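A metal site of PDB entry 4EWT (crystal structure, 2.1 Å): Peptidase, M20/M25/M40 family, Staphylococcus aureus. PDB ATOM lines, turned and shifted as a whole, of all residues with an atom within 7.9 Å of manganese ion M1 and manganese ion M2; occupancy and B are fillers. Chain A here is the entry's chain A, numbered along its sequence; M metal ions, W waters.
Manganese ion M2 is bound by the side-chain carboxylate (OE2) of Glu 139 (2.2 Å), water W2 (2.4 Å), the side-chain sulfur (SG) of Cys 103 (2.4 Å) and a ring nitrogen (NE2) of His 362 (2.5 Å). Manganese ion M2 has four donor atoms within binding distance. Slightly farther from manganese ion M2 lies OE1 of Glu 139 (2.8 Å).
Water W1 is bound to manganese ion M1 (2.3 Å). NE2 of His 164 is bound to manganese ion M1, 2.3 Å away. Manganese ion M1 is bound by a ring nitrogen (NE2) of His 105, at 2.3 Å. Manganese ion M1 is bound by water W2 (2.5 Å). SG of Cys 103 is bound to manganese ion M1 (2.6 Å).
The nearest printed residue that does not touch manganese ion M2 is Glu 138 (4.2 Å).
Glu 138 touches manganese ion M1. Within 4 Å of manganese ion M1: Cys 103, His 105, Glu 138, Glu 139 and His 164.
The backbone NH of Asp 334 sits at hydrogen-bond distance from the side-chain carboxylate of Glu 138 (3.2 Å). O of Asp 80 sits at hydrogen-bond distance from ND1 of His 105 (2.8 Å). N of Glu 138 sits at hydrogen-bond distance from OD2 of Asp 80, 2.8 Å away. The backbone NH (N) of Glu 139 is in hydrogen-bond range of the side-chain carboxylate (OD2) of Asp 80 (2.8 Å). A ring nitrogen (NE2) of His 105 sits close to the side-chain carboxylate (OD2) of Asp 78 (3.2 Å). The backbone carbonyl oxygen (O) of Ala 102 lies within hydrogen-bond range of the backbone NH (N) of His 362 (2.8 Å).
Water W2 lies within hydrogen-bond range of OE1 of Glu 138 (2.4 Å) and OE1 of Glu 139 (3.2 Å). Water W1 bridges OE1 of Glu 333 (2.7 Å) and OE1 of Glu 138 (3.5 Å).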
ATOM      1  N   ARG A  76     -36.471  18.887  -6.490  1.00  0.00           N
ATOM      2  CA  ARG A  76     -35.550  17.789  -6.750  1.00  0.00           C
ATOM      3  C   ARG A  76     -34.102  18.110  -6.372  1.00  0.00           C
ATOM      4  O   ARG A  76     -33.595  19.183  -6.698  1.00  0.00           O
ATOM      5  CB  ARG A  76     -35.666  17.361  -8.217  1.00  0.00           C
ATOM      6  CG  ARG A  76     -34.788  16.214  -8.639  1.00  0.00           C
ATOM      7  CD  ARG A  76     -33.408  16.679  -9.081  1.00  0.00           C
ATOM      8  NE  ARG A  76     -32.837  15.695  -9.988  1.00  0.00           N
ATOM      9  CZ  ARG A  76     -31.843  15.934 -10.844  1.00  0.00           C
ATOM     10  NH1 ARG A  76     -31.270  17.145 -10.930  1.00  0.00           N
ATOM     11  NH2 ARG A  76     -31.435  14.954 -11.633  1.00  0.00           N
ATOM     12  N   ASP A  78     -30.308  15.840  -6.367  1.00  0.00           N
ATOM     13  CA  ASP A  78     -29.574  14.588  -6.613  1.00  0.00           C
ATOM     14  C   ASP A  78     -28.432  14.416  -5.608  1.00  0.00           C
ATOM     15  O   ASP A  78     -27.966  15.394  -5.003  1.00  0.00           O
ATOM     16  CB  ASP A  78     -29.088  14.468  -8.074  1.00  0.00           C
ATOM     17  CG  ASP A  78     -28.573  15.783  -8.647  1.00  0.00           C
ATOM     18  OD1 ASP A  78     -28.452  16.795  -7.917  1.00  0.00           O
ATOM     19  OD2 ASP A  78     -28.271  15.813  -9.851  1.00  0.00           O
ATOM     20  N   ASP A  80     -25.752  11.490  -5.960  1.00  0.00           N
ATOM     21  CA  ASP A  80     -24.639  10.632  -6.383  1.00  0.00           C
ATOM     22  C   ASP A  80     -23.371  11.449  -6.657  1.00  0.00           C
ATOM     23  O   ASP A  80     -23.452  12.631  -7.020  1.00  0.00           O
ATOM     24  CB  ASP A  80     -24.995   9.771  -7.609  1.00  0.00           C
ATOM     25  CG  ASP A  80     -25.406  10.610  -8.830  1.00  0.00           C
ATOM     26  OD1 ASP A  80     -25.986  11.710  -8.672  1.00  0.00           O
ATOM     27  OD2 ASP A  80     -25.162  10.138  -9.962  1.00  0.00           O
ATOM     28  N   ALA A  81     -22.229  10.814  -6.457  1.00  0.00           N
ATOM     29  CA  ALA A  81     -20.922  11.435  -6.721  1.00  0.00           C
ATOM     30  C   ALA A  81     -20.278  10.835  -7.979  1.00  0.00           C
ATOM     31  O   ALA A  81     -20.918  10.057  -8.682  1.00  0.00           O
ATOM     32  CB  ALA A  81     -20.021  11.279  -5.522  1.00  0.00           C
ATOM     33  N   LEU A  82     -19.023  11.188  -8.239  1.00  0.00           N
ATOM     34  CA  LEU A  82     -18.322  10.797  -9.476  1.00  0.00           C
ATOM     35  C   LEU A  82     -17.008  10.045  -9.216  1.00  0.00           C
ATOM     36  O   LEU A  82     -16.410  10.198  -8.149  1.00  0.00           O
ATOM     37  CB  LEU A  82     -18.041  12.040 -10.321  1.00  0.00           C
ATOM     38  CG  LEU A  82     -19.216  12.731 -11.004  1.00  0.00           C
ATOM     39  CD1 LEU A  82     -18.921  14.210 -11.171  1.00  0.00           C
ATOM     40  CD2 LEU A  82     -19.509  12.077 -12.344  1.00  0.00           C
ATOM     41  N   ILE A  84     -13.786  10.345  -9.385  1.00  0.00           N
ATOM     42  CA  ILE A  84     -12.763  11.378  -9.527  1.00  0.00           C
ATOM     43  C   ILE A  84     -11.945  11.505  -8.232  1.00  0.00           C
ATOM     44  O   ILE A  84     -12.524  11.561  -7.142  1.00  0.00           O
ATOM     45  CB  ILE A  84     -13.401  12.752  -9.895  1.00  0.00           C
ATOM     46  CG1 ILE A  84     -13.970  12.721 -11.327  1.00  0.00           C
ATOM     47  CG2 ILE A  84     -12.401  13.897  -9.741  1.00  0.00           C
ATOM     48  CD1 ILE A  84     -15.111  13.674 -11.554  1.00  0.00           C
ATOM     49  N   ALA A 102     -17.973  16.082  -7.263  1.00  0.00           N
ATOM     50  CA  ALA A 102     -17.415  17.080  -8.180  1.00  0.00           C
ATOM     51  C   ALA A 102     -18.466  17.856  -8.987  1.00  0.00           C
ATOM     52  O   ALA A 102     -18.106  18.561  -9.935  1.00  0.00           O
ATOM     53  CB  ALA A 102     -16.394  16.404  -9.131  1.00  0.00           C
ATOM     54  N   CYS A 103     -19.735  17.730  -8.600  1.00  0.00           N
ATOM     55  CA  CYS A 103     -20.846  18.421  -9.304  1.00  0.00           C
ATOM     56  C   CYS A 103     -21.808  19.141  -8.347  1.00  0.00           C
ATOM     57  O   CYS A 103     -22.848  19.650  -8.770  1.00  0.00           O
ATOM     58  CB  CYS A 103     -21.624  17.430 -10.190  1.00  0.00           C
ATOM     59  SG  CYS A 103     -22.383  18.168 -11.671  1.00  0.00           S
ATOM     60  N   GLY A 104     -21.459  19.186  -7.067  1.00  0.00           N
ATOM     61  CA  GLY A 104     -22.212  19.941  -6.068  1.00  0.00           C
ATOM     62  C   GLY A 104     -23.470  19.240  -5.598  1.00  0.00           C
ATOM     63  O   GLY A 104     -24.341  19.881  -4.999  1.00  0.00           O
ATOM     64  N   HIS A 105     -23.566  17.936  -5.845  1.00  0.00           N
ATOM     65  CA  HIS A 105     -24.726  17.145  -5.426  1.00  0.00           C
ATOM     66  C   HIS A 105     -24.824  17.049  -3.901  1.00  0.00           C
ATOM     67  O   HIS A 105     -25.919  16.947  -3.343  1.00  0.00           O
ATOM     68  CB  HIS A 105     -24.670  15.735  -6.040  1.00  0.00           C
ATOM     69  CG  HIS A 105     -24.865  15.709  -7.525  1.00  0.00           C
ATOM     70  ND1 HIS A 105     -25.042  14.534  -8.213  1.00  0.00           N
ATOM     71  CD2 HIS A 105     -24.908  16.698  -8.448  1.00  0.00           C
ATOM     72  CE1 HIS A 105     -25.188  14.793  -9.501  1.00  0.00           C
ATOM     73  NE2 HIS A 105     -25.106  16.106  -9.668  1.00  0.00           N
ATOM     74  N   HIS A 108     -26.512  20.278  -3.179  1.00  0.00           N
ATOM     75  CA  HIS A 108     -27.933  20.145  -3.486  1.00  0.00           C
ATOM     76  C   HIS A 108     -28.696  19.416  -2.368  1.00  0.00           C
ATOM     77  O   HIS A 108     -29.779  19.838  -1.961  1.00  0.00           O
ATOM     78  CB  HIS A 108     -28.157  19.453  -4.823  1.00  0.00           C
ATOM     79  CG  HIS A 108     -27.495  20.137  -5.977  1.00  0.00           C
ATOM     80  ND1 HIS A 108     -27.152  19.482  -7.138  1.00  0.00           N
ATOM     81  CD2 HIS A 108     -27.109  21.427  -6.155  1.00  0.00           C
ATOM     82  CE1 HIS A 108     -26.580  20.333  -7.979  1.00  0.00           C
ATOM     83  NE2 HIS A 108     -26.543  21.519  -7.400  1.00  0.00           N
ATOM     84  N   GLU A 138     -27.751  10.151 -10.940  1.00  0.00           N
ATOM     85  CA  GLU A 138     -27.912  11.177 -11.978  1.00  0.00           C
ATOM     86  C   GLU A 138     -26.803  11.098 -13.044  1.00  0.00           C
ATOM     87  O   GLU A 138     -27.061  11.321 -14.220  1.00  0.00           O
ATOM     88  CB  GLU A 138     -27.957  12.582 -11.338  1.00  0.00           C
ATOM     89  CG  GLU A 138     -28.285  13.740 -12.302  1.00  0.00           C
ATOM     90  CD  GLU A 138     -27.113  14.192 -13.164  1.00  0.00           C
ATOM     91  OE1 GLU A 138     -25.955  14.142 -12.690  1.00  0.00           O
ATOM     92  OE2 GLU A 138     -27.350  14.598 -14.331  1.00  0.00           O
ATOM     93  N   GLU A 139     -25.593  10.766 -12.622  1.00  0.00           N
ATOM     94  CA  GLU A 139     -24.389  10.936 -13.441  1.00  0.00           C
ATOM     95  C   GLU A 139     -24.142   9.884 -14.517  1.00  0.00           C
ATOM     96  O   GLU A 139     -23.480  10.164 -15.526  1.00  0.00           O
ATOM     97  CB  GLU A 139     -23.148  11.053 -12.550  1.00  0.00           C
ATOM     98  CG  GLU A 139     -23.151  12.292 -11.670  1.00  0.00           C
ATOM     99  CD  GLU A 139     -22.894  13.585 -12.448  1.00  0.00           C
ATOM    100  OE1 GLU A 139     -22.887  13.571 -13.697  1.00  0.00           O
ATOM    101  OE2 GLU A 139     -22.691  14.626 -11.788  1.00  0.00           O
ATOM    102  N   VAL A 163     -32.769  22.730  -8.907  1.00  0.00           N
ATOM    103  CA  VAL A 163     -31.740  23.743  -8.861  1.00  0.00           C
ATOM    104  C   VAL A 163     -30.419  23.030  -8.995  1.00  0.00           C
ATOM    105  O   VAL A 163     -30.235  21.941  -8.464  1.00  0.00           O
ATOM    106  CB  VAL A 163     -31.789  24.555  -7.532  1.00  0.00           C
ATOM    107  CG1 VAL A 163     -30.457  25.270  -7.281  1.00  0.00           C
ATOM    108  CG2 VAL A 163     -32.911  25.552  -7.564  1.00  0.00           C
ATOM    109  N   HIS A 164     -29.499  23.649  -9.748  1.00  0.00           N
ATOM    110  CA  HIS A 164     -28.124  23.201  -9.795  1.00  0.00           C
ATOM    111  C   HIS A 164     -27.233  24.385  -9.453  1.00  0.00           C
ATOM    112  O   HIS A 164     -27.391  25.479 -10.018  1.00  0.00           O
ATOM    113  CB  HIS A 164     -27.780  22.666 -11.185  1.00  0.00           C
ATOM    114  CG  HIS A 164     -26.737  21.594 -11.179  1.00  0.00           C
ATOM    115  ND1 HIS A 164     -25.419  21.847 -10.891  1.00  0.00           N
ATOM    116  CD2 HIS A 164     -26.824  20.269 -11.419  1.00  0.00           C
ATOM    117  CE1 HIS A 164     -24.731  20.728 -10.967  1.00  0.00           C
ATOM    118  NE2 HIS A 164     -25.560  19.748 -11.298  1.00  0.00           N
ATOM    119  N   VAL A 165     -26.311  24.168  -8.509  1.00  0.00           N
ATOM    120  CA  VAL A 165     -25.223  25.114  -8.259  1.00  0.00           C
ATOM    121  C   VAL A 165     -24.276  25.141  -9.454  1.00  0.00           C
ATOM    122  O   VAL A 165     -23.954  24.103 -10.037  1.00  0.00           O
ATOM    123  CB  VAL A 165     -24.425  24.763  -6.981  1.00  0.00           C
ATOM    124  CG1 VAL A 165     -25.269  24.966  -5.725  1.00  0.00           C
ATOM    125  CG2 VAL A 165     -23.861  23.314  -7.049  1.00  0.00           C
ATOM    126  N   MET A 166     -23.858  26.347  -9.834  1.00  0.00           N
ATOM    127  CA  MET A 166     -22.952  26.533 -10.951  1.00  0.00           C
ATOM    128  C   MET A 166     -21.651  27.189 -10.518  1.00  0.00           C
ATOM    129  O   MET A 166     -21.604  28.393 -10.259  1.00  0.00           O
ATOM    130  CB  MET A 166     -23.626  27.351 -12.047  1.00  0.00           C
ATOM    131  CG  MET A 166     -24.906  26.731 -12.584  1.00  0.00           C
ATOM    132  SD  MET A 166     -24.670  25.113 -13.330  1.00  0.00           S
ATOM    133  CE  MET A 166     -24.337  25.567 -15.025  1.00  0.00           C
ATOM    134  N   GLN A 182     -30.441  22.619 -21.525  1.00  0.00           N
ATOM    135  CA  GLN A 182     -29.287  21.697 -21.508  1.00  0.00           C
ATOM    136  C   GLN A 182     -29.452  20.620 -22.567  1.00  0.00           C
ATOM    137  O   GLN A 182     -30.557  20.220 -22.881  1.00  0.00           O
ATOM    138  CB  GLN A 182     -29.060  21.115 -20.104  1.00  0.00           C
ATOM    139  CG  GLN A 182     -28.509  22.178 -19.169  1.00  0.00           C
ATOM    140  CD  GLN A 182     -28.052  21.705 -17.813  1.00  0.00           C
ATOM    141  OE1 GLN A 182     -28.330  22.358 -16.820  1.00  0.00           O
ATOM    142  NE2 GLN A 182     -27.313  20.602 -17.759  1.00  0.00           N
ATOM    143  N   PRO A 331     -23.560  20.727 -20.466  1.00  0.00           N
ATOM    144  CA  PRO A 331     -23.695  19.326 -20.034  1.00  0.00           C
ATOM    145  C   PRO A 331     -25.124  18.768 -20.128  1.00  0.00           C
ATOM    146  O   PRO A 331     -26.094  19.528 -20.176  1.00  0.00           O
ATOM    147  CB  PRO A 331     -23.223  19.361 -18.583  1.00  0.00           C
ATOM    148  CG  PRO A 331     -23.478  20.717 -18.127  1.00  0.00           C
ATOM    149  CD  PRO A 331     -23.324  21.616 -19.325  1.00  0.00           C
ATOM    150  N   SER A 332     -25.251  17.447 -20.154  1.00  0.00           N
ATOM    151  CA  SER A 332     -26.561  16.830 -20.130  1.00  0.00           C
ATOM    152  C   SER A 332     -26.913  16.598 -18.668  1.00  0.00           C
ATOM    153  O   SER A 332     -26.039  16.591 -17.790  1.00  0.00           O
ATOM    154  CB  SER A 332     -26.598  15.534 -20.957  1.00  0.00           C
ATOM    155  OG  SER A 332     -26.406  14.411 -20.115  1.00  0.00           O
ATOM    156  N   GLU A 333     -28.202  16.426 -18.399  1.00  0.00           N
ATOM    157  CA  GLU A 333     -28.713  16.402 -17.048  1.00  0.00           C
ATOM    158  C   GLU A 333     -29.955  15.514 -17.065  1.00  0.00           C
ATOM    159  O   GLU A 333     -30.839  15.702 -17.913  1.00  0.00           O
ATOM    160  CB  GLU A 333     -29.055  17.847 -16.639  1.00  0.00           C
ATOM    161  CG  GLU A 333     -29.934  18.021 -15.420  1.00  0.00           C
ATOM    162  CD  GLU A 333     -29.335  17.460 -14.166  1.00  0.00           C
ATOM    163  OE1 GLU A 333     -28.203  17.866 -13.816  1.00  0.00           O
ATOM    164  OE2 GLU A 333     -29.997  16.612 -13.520  1.00  0.00           O
ATOM    165  N   ASP A 334     -30.031  14.543 -16.149  1.00  0.00           N
ATOM    166  CA  ASP A 334     -31.178  13.638 -16.179  1.00  0.00           C
ATOM    167  C   ASP A 334     -32.479  14.190 -15.583  1.00  0.00           C
ATOM    168  O   ASP A 334     -33.534  13.568 -15.710  1.00  0.00           O
ATOM    169  CB  ASP A 334     -30.823  12.207 -15.731  1.00  0.00           C
ATOM    170  CG  ASP A 334     -31.146  11.929 -14.274  1.00  0.00           C
ATOM    171  OD1 ASP A 334     -31.343  12.872 -13.482  1.00  0.00           O
ATOM    172  OD2 ASP A 334     -31.178  10.724 -13.921  1.00  0.00           O
ATOM    173  N   PHE A 346     -35.669  23.976 -14.416  1.00  0.00           N
ATOM    174  CA  PHE A 346     -34.382  23.672 -13.803  1.00  0.00           C
ATOM    175  C   PHE A 346     -33.640  24.980 -13.796  1.00  0.00           C
ATOM    176  O   PHE A 346     -33.391  25.554 -14.861  1.00  0.00           O
ATOM    177  CB  PHE A 346     -33.658  22.618 -14.641  1.00  0.00           C
ATOM    178  CG  PHE A 346     -32.452  22.002 -13.973  1.00  0.00           C
ATOM    179  CD1 PHE A 346     -32.590  21.224 -12.814  1.00  0.00           C
ATOM    180  CD2 PHE A 346     -31.193  22.171 -14.519  1.00  0.00           C
ATOM    181  CE1 PHE A 346     -31.465  20.631 -12.216  1.00  0.00           C
ATOM    182  CE2 PHE A 346     -30.062  21.572 -13.932  1.00  0.00           C
ATOM    183  CZ  PHE A 346     -30.199  20.806 -12.779  1.00  0.00           C
ATOM    184  N   HIS A 361     -17.202  21.952 -13.396  1.00  0.00           N
ATOM    185  CA  HIS A 361     -17.720  20.686 -12.851  1.00  0.00           C
ATOM    186  C   HIS A 361     -16.973  19.458 -13.356  1.00  0.00           C
ATOM    187  O   HIS A 361     -16.458  19.452 -14.487  1.00  0.00           O
ATOM    188  CB  HIS A 361     -19.206  20.550 -13.162  1.00  0.00           C
ATOM    189  CG  HIS A 361     -20.064  21.538 -12.427  1.00  0.00           C
ATOM    190  ND1 HIS A 361     -19.968  22.902 -12.614  1.00  0.00           N
ATOM    191  CD2 HIS A 361     -21.047  21.358 -11.510  1.00  0.00           C
ATOM    192  CE1 HIS A 361     -20.840  23.512 -11.833  1.00  0.00           C
ATOM    193  NE2 HIS A 361     -21.499  22.601 -11.153  1.00  0.00           N
ATOM    194  N   HIS A 362     -16.914  18.431 -12.509  1.00  0.00           N
ATOM    195  CA  HIS A 362     -16.181  17.175 -12.778  1.00  0.00           C
ATOM    196  C   HIS A 362     -14.655  17.268 -12.696  1.00  0.00           C
ATOM    197  O   HIS A 362     -13.969  16.254 -12.767  1.00  0.00           O
ATOM    198  CB  HIS A 362     -16.553  16.598 -14.155  1.00  0.00           C
ATOM    199  CG  HIS A 362     -17.945  16.078 -14.242  1.00  0.00           C
ATOM    200  ND1 HIS A 362     -18.254  14.855 -14.796  1.00  0.00           N
ATOM    201  CD2 HIS A 362     -19.130  16.621 -13.853  1.00  0.00           C
ATOM    202  CE1 HIS A 362     -19.553  14.659 -14.746  1.00  0.00           C
ATOM    203  NE2 HIS A 362     -20.115  15.719 -14.172  1.00  0.00           N
ATOM    204  N   PHE A 366     -12.650  21.168  -8.471  1.00  0.00           N
ATOM    205  CA  PHE A 366     -13.999  21.743  -8.366  1.00  0.00           C
ATOM    206  C   PHE A 366     -14.312  22.250  -6.963  1.00  0.00           C
ATOM    207  O   PHE A 366     -14.135  21.533  -5.984  1.00  0.00           O
ATOM    208  CB  PHE A 366     -15.033  20.687  -8.785  1.00  0.00           C
ATOM    209  CG  PHE A 366     -16.467  21.095  -8.572  1.00  0.00           C
ATOM    210  CD1 PHE A 366     -17.146  21.833  -9.540  1.00  0.00           C
ATOM    211  CD2 PHE A 366     -17.154  20.723  -7.413  1.00  0.00           C
ATOM    212  CE1 PHE A 366     -18.477  22.209  -9.355  1.00  0.00           C
ATOM    213  CE2 PHE A 366     -18.479  21.097  -7.215  1.00  0.00           C
ATOM    214  CZ  PHE A 366     -19.143  21.829  -8.190  1.00  0.00           C
HETATM  215 MN    MN M   1     -24.902  17.576 -11.408  1.00  0.00          MN
HETATM  216 MN    MN M   2     -22.348  16.253 -13.183  1.00  0.00          MN
HETATM  217  O   HOH W   1     -27.123  17.165 -11.459  1.00  0.00           O
HETATM  218  O   HOH W   2     -24.762  16.125 -13.411  1.00  0.00           O
HETATM  219  O   HOH W   3     -21.825  18.862 -15.185  1.00  0.00           O
